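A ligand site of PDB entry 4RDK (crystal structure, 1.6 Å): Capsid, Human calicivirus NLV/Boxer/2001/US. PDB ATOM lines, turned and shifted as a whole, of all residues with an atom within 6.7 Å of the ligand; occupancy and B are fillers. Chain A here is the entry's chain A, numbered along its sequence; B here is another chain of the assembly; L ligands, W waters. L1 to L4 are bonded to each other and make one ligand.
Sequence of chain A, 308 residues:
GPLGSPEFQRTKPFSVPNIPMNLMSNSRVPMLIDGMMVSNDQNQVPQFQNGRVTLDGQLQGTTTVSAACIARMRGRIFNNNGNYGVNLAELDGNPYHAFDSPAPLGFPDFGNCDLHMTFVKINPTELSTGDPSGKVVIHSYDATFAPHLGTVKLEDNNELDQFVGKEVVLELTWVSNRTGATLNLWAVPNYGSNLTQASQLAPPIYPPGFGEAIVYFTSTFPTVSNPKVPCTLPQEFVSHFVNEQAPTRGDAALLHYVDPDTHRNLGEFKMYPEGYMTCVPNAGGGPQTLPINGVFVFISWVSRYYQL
Water W2 lies within hydrogen-bond range of an oxygen (O5) of LG2 L2 and the side-chain amide nitrogen (ND2) of Asn 177.
Water W13 bridges the side-chain carboxylate (OD2) of Asp 131 of chain B (2.7 Å) and an oxygen (O3) of LIG L1 (2.8 Å).
Water W9 lies within hydrogen-bond range of the side-chain amide oxygen (OD1) of Asn 177, the backbone carbonyl oxygen (O) of Val 224 and an oxygen (O3) of LG4 L4.
Water W12 bridges an oxygen (O2) of LG4 L4 (2.8 Å) and the backbone carbonyl oxygen of Ser 128 of chain B (2.9 Å).
Trp 174 touches the ligand.
Val 224 touches the ligand.
CA of Thr 129 of chain B touches O3 of LG4 L4 (3.7 Å).
Hydrophobic or aromatic side chains within 4 Å of the ligand: His 116, Trp 174 and Val 224.
The nearest printed residue that does not touch the ligand is Ser 128 of chain B (4.3 Å).
ND2 of Asn 177 sits at hydrogen-bond distance from O of Ala 181, 3.0 Å away.
N of Asp 114 is in hydrogen-bond range of O of Ser 176, 2.9 Å away.
A ring nitrogen (NE2) of His 116 sits at hydrogen-bond distance from the side-chain hydroxyl (OG) of Ser 176 (2.8 Å).
OD1 of Asp 114 sits at hydrogen-bond distance from OH of Tyr 141, 2.7 Å away.
OD1 of Asp 131 of chain B is in hydrogen-bond range of NE1 of Trp 174 (3.4 Å).
The backbone carbonyl oxygen (O) of Trp 174 sits at hydrogen-bond distance from the backbone NH (N) of His 116 (2.9 Å).
The backbone NH (N) of Val 224 is in hydrogen-bond range of the backbone carbonyl oxygen (O) of Val 175, 2.9 Å away.
O of Asn 177 lies within hydrogen-bond range of O3 of LG2 L2 (2.7 Å).
The side-chain amide oxygen of Asn 177 is in hydrogen-bond range of an oxygen (O2) of LG4 L4.
OG of Ser 176 is in hydrogen-bond range of O3 of LG2 L2 (2.8 Å).
An oxygen (O2) of LG2 L2 is in hydrogen-bond range of the side-chain carboxylate (OD2) of Asp 114 (2.9 Å).
The backbone NH (N) of Gly 130 of chain B lies within hydrogen-bond range of an oxygen (O4) of LG4 L4 (3.0 Å).
The side-chain hydroxyl (OG1) of Thr 179 is in hydrogen-bond range of an oxygen (O5) of LG2 L2, 3.2 Å away.
The side-chain carboxylate (OD2) of Asp 131 of chain B lies close to an oxygen (O3) of LIG L1 (3.4 Å).
A ring nitrogen (NE2) of His 116 lies close to an oxygen (O2) of LG2 L2, 3.4 Å away.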
ATOM      1  N   ASP A 114       1.336   9.558   8.540  1.00  0.00           N
ATOM      2  CA  ASP A 114       1.053   8.358   9.306  1.00  0.00           C
ATOM      3  C   ASP A 114       2.355   7.613   9.591  1.00  0.00           C
ATOM      4  O   ASP A 114       3.045   7.172   8.660  1.00  0.00           O
ATOM      5  CB  ASP A 114       0.101   7.442   8.526  1.00  0.00           C
ATOM      6  CG  ASP A 114      -1.332   7.954   8.501  1.00  0.00           C
ATOM      7  OD1 ASP A 114      -1.584   9.092   8.971  1.00  0.00           O
ATOM      8  OD2 ASP A 114      -2.202   7.219   7.995  1.00  0.00           O
ATOM      9  N   HIS A 116       4.068   4.425  10.852  1.00  0.00           N
ATOM     10  CA  HIS A 116       3.789   3.009  11.107  1.00  0.00           C
ATOM     11  C   HIS A 116       4.925   2.458  11.950  1.00  0.00           C
ATOM     12  O   HIS A 116       6.047   2.302  11.452  1.00  0.00           O
ATOM     13  CB  HIS A 116       3.618   2.251   9.786  1.00  0.00           C
ATOM     14  CG  HIS A 116       2.526   2.807   8.927  1.00  0.00           C
ATOM     15  ND1 HIS A 116       1.246   2.285   8.906  1.00  0.00           N
ATOM     16  CD2 HIS A 116       2.517   3.863   8.068  1.00  0.00           C
ATOM     17  CE1 HIS A 116       0.497   2.983   8.072  1.00  0.00           C
ATOM     18  NE2 HIS A 116       1.246   3.945   7.541  1.00  0.00           N
ATOM     19  N   VAL A 137      -0.100   2.420  14.406  1.00  0.00           N
ATOM     20  CA  VAL A 137       0.027   3.643  13.632  1.00  0.00           C
ATOM     21  C   VAL A 137      -0.112   4.834  14.566  1.00  0.00           C
ATOM     22  O   VAL A 137      -1.000   4.849  15.432  1.00  0.00           O
ATOM     23  CB  VAL A 137      -1.056   3.735  12.535  1.00  0.00           C
ATOM     24  CG1 VAL A 137      -0.935   5.058  11.769  1.00  0.00           C
ATOM     25  CG2 VAL A 137      -0.946   2.553  11.592  1.00  0.00           C
ATOM     26  N   HIS A 139      -0.482   9.019  14.211  1.00  0.00           N
ATOM     27  CA  HIS A 139      -0.624  10.215  13.389  1.00  0.00           C
ATOM     28  C   HIS A 139       0.228  11.343  13.939  1.00  0.00           C
ATOM     29  O   HIS A 139       0.098  11.699  15.109  1.00  0.00           O
ATOM     30  CB  HIS A 139      -2.070  10.703  13.408  1.00  0.00           C
ATOM     31  CG  HIS A 139      -3.031   9.760  12.760  1.00  0.00           C
ATOM     32  ND1 HIS A 139      -4.397   9.928  12.857  1.00  0.00           N
ATOM     33  CD2 HIS A 139      -2.839   8.672  11.975  1.00  0.00           C
ATOM     34  CE1 HIS A 139      -5.004   8.968  12.181  1.00  0.00           C
ATOM     35  NE2 HIS A 139      -4.082   8.195  11.630  1.00  0.00           N
ATOM     36  N   TYR A 141      -0.239  14.379  13.626  1.00  0.00           N
ATOM     37  CA  TYR A 141      -1.193  15.456  13.386  1.00  0.00           C
ATOM     38  C   TYR A 141      -2.417  15.302  14.278  1.00  0.00           C
ATOM     39  O   TYR A 141      -2.561  14.272  14.947  1.00  0.00           O
ATOM     40  CB  TYR A 141      -1.618  15.509  11.910  1.00  0.00           C
ATOM     41  CG  TYR A 141      -2.165  14.222  11.326  1.00  0.00           C
ATOM     42  CD1 TYR A 141      -3.531  13.940  11.337  1.00  0.00           C
ATOM     43  CD2 TYR A 141      -1.321  13.289  10.734  1.00  0.00           C
ATOM     44  CE1 TYR A 141      -4.035  12.760  10.792  1.00  0.00           C
ATOM     45  CE2 TYR A 141      -1.809  12.114  10.184  1.00  0.00           C
ATOM     46  CZ  TYR A 141      -3.160  11.856  10.206  1.00  0.00           C
ATOM     47  OH  TYR A 141      -3.656  10.686   9.654  1.00  0.00           O
ATOM     48  N   TRP A 174       7.721   2.297   8.691  1.00  0.00           N
ATOM     49  CA  TRP A 174       7.444   2.957   7.422  1.00  0.00           C
ATOM     50  C   TRP A 174       6.515   4.149   7.628  1.00  0.00           C
ATOM     51  O   TRP A 174       5.962   4.337   8.717  1.00  0.00           O
ATOM     52  CB  TRP A 174       6.924   1.969   6.348  1.00  0.00           C
ATOM     53  CG  TRP A 174       5.573   1.321   6.600  1.00  0.00           C
ATOM     54  CD1 TRP A 174       5.274   0.333   7.504  1.00  0.00           C
ATOM     55  CD2 TRP A 174       4.353   1.599   5.896  1.00  0.00           C
ATOM     56  NE1 TRP A 174       3.928  -0.004   7.413  1.00  0.00           N
ATOM     57  CE2 TRP A 174       3.352   0.754   6.426  1.00  0.00           C
ATOM     58  CE3 TRP A 174       4.022   2.480   4.861  1.00  0.00           C
ATOM     59  CZ2 TRP A 174       2.040   0.780   5.970  1.00  0.00           C
ATOM     60  CZ3 TRP A 174       2.712   2.492   4.403  1.00  0.00           C
ATOM     61  CH2 TRP A 174       1.739   1.658   4.956  1.00  0.00           C
ATOM     62  N   VAL A 175       6.363   4.947   6.585  1.00  0.00           N
ATOM     63  CA  VAL A 175       5.572   6.173   6.663  1.00  0.00           C
ATOM     64  C   VAL A 175       4.663   6.284   5.449  1.00  0.00           C
ATOM     65  O   VAL A 175       5.079   5.949   4.344  1.00  0.00           O
ATOM     66  CB  VAL A 175       6.496   7.419   6.669  1.00  0.00           C
ATOM     67  CG1 VAL A 175       5.666   8.701   6.702  1.00  0.00           C
ATOM     68  CG2 VAL A 175       7.462   7.378   7.844  1.00  0.00           C
ATOM     69  N   SER A 176       3.430   6.740   5.646  1.00  0.00           N
ATOM     70  CA  SER A 176       2.539   7.026   4.519  1.00  0.00           C
ATOM     71  C   SER A 176       1.857   8.382   4.687  1.00  0.00           C
ATOM     72  O   SER A 176       1.905   8.982   5.767  1.00  0.00           O
ATOM     73  CB  SER A 176       1.495   5.913   4.347  1.00  0.00           C
ATOM     74  OG  SER A 176       0.672   5.788   5.499  1.00  0.00           O
ATOM     75  N   ASN A 177       1.225   8.860   3.619  1.00  0.00           N
ATOM     76  CA  ASN A 177       0.546  10.136   3.683  1.00  0.00           C
ATOM     77  C   ASN A 177      -0.725  10.094   4.529  1.00  0.00           C
ATOM     78  O   ASN A 177      -1.393   9.053   4.638  1.00  0.00           O
ATOM     79  CB  ASN A 177       0.229  10.665   2.285  1.00  0.00           C
ATOM     80  CG  ASN A 177      -0.789   9.809   1.548  1.00  0.00           C
ATOM     81  OD1 ASN A 177      -0.473   8.702   1.119  1.00  0.00           O
ATOM     82  ND2 ASN A 177      -2.008  10.322   1.394  1.00  0.00           N
ATOM     83  N   ARG A 178      -1.044  11.229   5.126  1.00  0.00           N
ATOM     84  CA  ARG A 178      -2.321  11.439   5.775  1.00  0.00           C
ATOM     85  C   ARG A 178      -3.394  11.495   4.685  1.00  0.00           C
ATOM     86  O   ARG A 178      -3.180  12.087   3.632  1.00  0.00           O
ATOM     87  CB  ARG A 178      -2.281  12.776   6.524  1.00  0.00           C
ATOM     88  CG  ARG A 178      -3.616  13.311   6.940  1.00  0.00           C
ATOM     89  CD  ARG A 178      -3.450  14.618   7.695  1.00  0.00           C
ATOM     90  NE  ARG A 178      -4.724  15.063   8.233  1.00  0.00           N
ATOM     91  CZ  ARG A 178      -4.892  16.140   8.980  1.00  0.00           C
ATOM     92  NH1 ARG A 178      -3.855  16.896   9.290  1.00  0.00           N
ATOM     93  NH2 ARG A 178      -6.108  16.464   9.426  1.00  0.00           N
ATOM     94  N   THR A 179      -4.539  10.853   4.925  1.00  0.00           N
ATOM     95  CA  THR A 179      -5.627  10.941   3.956  1.00  0.00           C
ATOM     96  C   THR A 179      -5.928  12.392   3.631  1.00  0.00           C
ATOM     97  O   THR A 179      -6.053  13.224   4.536  1.00  0.00           O
ATOM     98  CB  THR A 179      -6.903  10.267   4.479  1.00  0.00           C
ATOM     99  OG1 THR A 179      -6.628   8.899   4.791  1.00  0.00           O
ATOM    100  CG2 THR A 179      -7.992  10.329   3.427  1.00  0.00           C
ATOM    101  N   GLY A 180      -6.019  12.711   2.343  1.00  0.00           N
ATOM    102  CA  GLY A 180      -6.348  14.059   1.920  1.00  0.00           C
ATOM    103  C   GLY A 180      -5.159  14.980   1.756  1.00  0.00           C
ATOM    104  O   GLY A 180      -5.321  16.135   1.373  1.00  0.00           O
ATOM    105  N   ALA A 181      -3.963  14.473   2.044  1.00  0.00           N
ATOM    106  CA  ALA A 181      -2.746  15.275   1.940  1.00  0.00           C
ATOM    107  C   ALA A 181      -1.632  14.515   1.233  1.00  0.00           C
ATOM    108  O   ALA A 181      -1.678  13.289   1.125  1.00  0.00           O
ATOM    109  CB  ALA A 181      -2.282  15.711   3.330  1.00  0.00           C
ATOM    110  N   VAL A 224       6.530   5.999   1.884  1.00  0.00           N
ATOM    111  CA  VAL A 224       5.804   5.585   0.697  1.00  0.00           C
ATOM    112  C   VAL A 224       5.233   6.784  -0.073  1.00  0.00           C
ATOM    113  O   VAL A 224       4.581   7.637   0.517  1.00  0.00           O
ATOM    114  CB  VAL A 224       4.711   4.558   1.057  1.00  0.00           C
ATOM    115  CG1 VAL A 224       3.843   4.232  -0.161  1.00  0.00           C
ATOM    116  CG2 VAL A 224       5.366   3.295   1.627  1.00  0.00           C
ATOM    117  N   SER A 225       5.492   6.799  -1.387  1.00  0.00           N
ATOM    118  CA  SER A 225       5.173   7.888  -2.318  1.00  0.00           C
ATOM    119  C   SER A 225       6.353   8.855  -2.519  1.00  0.00           C
ATOM    120  O   SER A 225       6.364   9.629  -3.475  1.00  0.00           O
ATOM    121  CB  SER A 225       3.887   8.653  -1.954  1.00  0.00           C
ATOM    122  OG  SER A 225       4.133   9.685  -1.023  1.00  0.00           O
ATOM    123  N   SER B 128       5.790   3.182  -3.950  1.00  0.00           N
ATOM    124  CA  SER B 128       4.943   4.266  -4.443  1.00  0.00           C
ATOM    125  C   SER B 128       3.587   4.315  -3.717  1.00  0.00           C
ATOM    126  O   SER B 128       3.043   5.399  -3.461  1.00  0.00           O
ATOM    127  CB  SER B 128       4.730   4.117  -5.951  1.00  0.00           C
ATOM    128  OG  SER B 128       3.872   5.116  -6.435  1.00  0.00           O
ATOM    129  N   THR B 129       3.048   3.146  -3.405  1.00  0.00           N
ATOM    130  CA  THR B 129       1.759   3.012  -2.727  1.00  0.00           C
ATOM    131  C   THR B 129       1.778   1.724  -1.925  1.00  0.00           C
ATOM    132  O   THR B 129       2.646   0.875  -2.111  1.00  0.00           O
ATOM    133  CB  THR B 129       0.591   2.888  -3.728  1.00  0.00           C
ATOM    134  OG1 THR B 129       0.754   1.679  -4.483  1.00  0.00           O
ATOM    135  CG2 THR B 129       0.550   4.066  -4.680  1.00  0.00           C
ATOM    136  N   GLY B 130       0.803   1.590  -1.025  1.00  0.00           N
ATOM    137  CA  GLY B 130       0.614   0.357  -0.286  1.00  0.00           C
ATOM    138  C   GLY B 130       1.552   0.155   0.897  1.00  0.00           C
ATOM    139  O   GLY B 130       2.450   0.960   1.146  1.00  0.00           O
ATOM    140  N   ASP B 131       1.320  -0.932   1.619  1.00  0.00           N
ATOM    141  CA  ASP B 131       2.085  -1.292   2.804  1.00  0.00           C
ATOM    142  C   ASP B 131       3.246  -2.202   2.374  1.00  0.00           C
ATOM    143  O   ASP B 131       3.024  -3.305   1.860  1.00  0.00           O
ATOM    144  CB  ASP B 131       1.153  -2.033   3.772  1.00  0.00           C
ATOM    145  CG  ASP B 131       1.824  -2.422   5.069  1.00  0.00           C
ATOM    146  OD1 ASP B 131       3.070  -2.391   5.144  1.00  0.00           O
ATOM    147  OD2 ASP B 131       1.108  -2.788   6.022  1.00  0.00           O
ATOM    148  N   PRO B 132       4.480  -1.718   2.544  1.00  0.00           N
ATOM    149  CA  PRO B 132       5.663  -2.465   2.082  1.00  0.00           C
ATOM    150  C   PRO B 132       6.194  -3.426   3.138  1.00  0.00           C
ATOM    151  O   PRO B 132       7.211  -4.080   2.896  1.00  0.00           O
ATOM    152  CB  PRO B 132       6.689  -1.354   1.856  1.00  0.00           C
ATOM    153  CG  PRO B 132       6.380  -0.377   2.944  1.00  0.00           C
ATOM    154  CD  PRO B 132       4.859  -0.410   3.115  1.00  0.00           C
HETATM  155  C1  LIG L   1      -2.053   1.751   5.498  1.00  0.00           C
HETATM  156  C2  LIG L   1      -2.267   0.723   6.576  1.00  0.00           C
HETATM  157  C3  LIG L   1      -3.354  -0.212   6.199  1.00  0.00           C
HETATM  158  C4  LIG L   1      -3.126  -0.831   4.921  1.00  0.00           C
HETATM  159  C5  LIG L   1      -2.865   0.198   3.861  1.00  0.00           C
HETATM  160  C6  LIG L   1      -2.501  -0.420   2.589  1.00  0.00           C
HETATM  161  O1  LIG L   1      -2.562   1.350   7.788  1.00  0.00           O
HETATM  162  O2  LIG L   1      -3.522  -1.207   7.225  1.00  0.00           O
HETATM  163  O3  LIG L   1      -2.006  -1.737   4.998  1.00  0.00           O
HETATM  164  O4  LIG L   1      -1.775   1.113   4.278  1.00  0.00           O
HETATM  165  C1  LG2 L   2      -4.087   3.861   3.574  1.00  0.00           C
HETATM  166  C2  LG2 L   2      -2.985   3.760   4.610  1.00  0.00           C
HETATM  167  C3  LG2 L   2      -2.961   4.886   5.492  1.00  0.00           C
HETATM  168  C4  LG2 L   2      -2.916   6.189   4.793  1.00  0.00           C
HETATM  169  C5  LG2 L   2      -4.054   6.264   3.781  1.00  0.00           C
HETATM  170  C6  LG2 L   2      -4.012   7.536   2.987  1.00  0.00           C
HETATM  171  O1  LG2 L   2      -3.198   2.519   5.372  1.00  0.00           O
HETATM  172  O2  LG2 L   2      -1.871   4.825   6.425  1.00  0.00           O
HETATM  173  O3  LG2 L   2      -1.695   6.376   4.145  1.00  0.00           O
HETATM  174  O4  LG2 L   2      -4.039   5.177   2.900  1.00  0.00           O
HETATM  175  O5  LG2 L   2      -5.166   7.755   2.185  1.00  0.00           O
HETATM  176  C1  LG3 L   3      -7.074   1.391   1.009  1.00  0.00           C
HETATM  177  C2  LG3 L   3      -5.996   1.654   2.018  1.00  0.00           C
HETATM  178  C3  LG3 L   3      -5.122   2.776   1.665  1.00  0.00           C
HETATM  179  C4  LG3 L   3      -4.619   2.638   0.330  1.00  0.00           C
HETATM  180  C5  LG3 L   3      -5.752   2.472  -0.624  1.00  0.00           C
HETATM  181  C6  LG3 L   3      -5.286   2.298  -2.023  1.00  0.00           C
HETATM  182  C7  LG3 L   3      -6.806   0.794   4.263  1.00  0.00           C
HETATM  183  C8  LG3 L   3      -7.455   1.028   5.609  1.00  0.00           C
HETATM  184  O1  LG3 L   3      -6.556   1.303  -0.288  1.00  0.00           O
HETATM  185  O2  LG3 L   3      -4.007   2.853   2.647  1.00  0.00           O
HETATM  186  O3  LG3 L   3      -3.811   3.840  -0.030  1.00  0.00           O
HETATM  187  O4  LG3 L   3      -4.701   1.067  -2.317  1.00  0.00           O
HETATM  188  O5  LG3 L   3      -6.429  -0.314   3.953  1.00  0.00           O
HETATM  189  N1  LG3 L   3      -6.638   1.877   3.354  1.00  0.00           N
HETATM  190  O6  LG3 L   3      -8.011   2.419   1.057  1.00  0.00           O
HETATM  191  C1  LG4 L   4      -2.667   3.610  -0.763  1.00  0.00           C
HETATM  192  C2  LG4 L   4      -2.221   4.904  -1.342  1.00  0.00           C
HETATM  193  C3  LG4 L   4      -1.843   5.836  -0.310  1.00  0.00           C
HETATM  194  C4  LG4 L   4      -0.820   5.281   0.589  1.00  0.00           C
HETATM  195  C5  LG4 L   4      -1.244   3.923   1.140  1.00  0.00           C
HETATM  196  C6  LG4 L   4      -0.162   3.336   1.999  1.00  0.00           C
HETATM  197  O1  LG4 L   4      -3.289   5.437  -2.154  1.00  0.00           O
HETATM  198  O2  LG4 L   4      -1.346   7.075  -0.893  1.00  0.00           O
HETATM  199  O3  LG4 L   4       0.413   5.175  -0.096  1.00  0.00           O
HETATM  200  O4  LG4 L   4      -1.583   3.045   0.101  1.00  0.00           O
HETATM  201  O   HOH W   1      -5.949  -2.058   1.774  1.00  0.00           O
HETATM  202  O   HOH W   2      -4.302   8.987  -0.014  1.00  0.00           O
HETATM  203  O   HOH W   3      -5.981  -1.738   8.133  1.00  0.00           O
HETATM  204  O   HOH W   4      -5.625   6.161  -0.398  1.00  0.00           O
HETATM  205  O   HOH W   5      -7.081  -2.484   5.537  1.00  0.00           O
HETATM  206  O   HOH W   6      -7.217   5.930   1.528  1.00  0.00           O
HETATM  207  O   HOH W   7      -1.954  -3.799   3.030  1.00  0.00           O
HETATM  208  O   HOH W   8      -7.757   4.470   4.023  1.00  0.00           O
HETATM  209  O   HOH W   9       1.884   7.249   1.089  1.00  0.00           O
HETATM  210  O   HOH W  10      -2.372  -0.340   9.986  1.00  0.00           O
HETATM  211  O   HOH W  11      -5.069   2.621   8.159  1.00  0.00           O
HETATM  212  O   HOH W  12       0.770   6.990  -2.774  1.00  0.00           O
HETATM  213  O   HOH W  13      -1.325  -3.255   7.204  1.00  0.00           O
HETATM  214  O   HOH W  14      -4.745  -1.273  -0.649  1.00  0.00           O
HETATM  215  O   HOH W  15      -3.424   4.751  -4.835  1.00  0.00           O
HETATM  216  O   HOH W  16      -3.351   8.215  -2.843  1.00  0.00           O
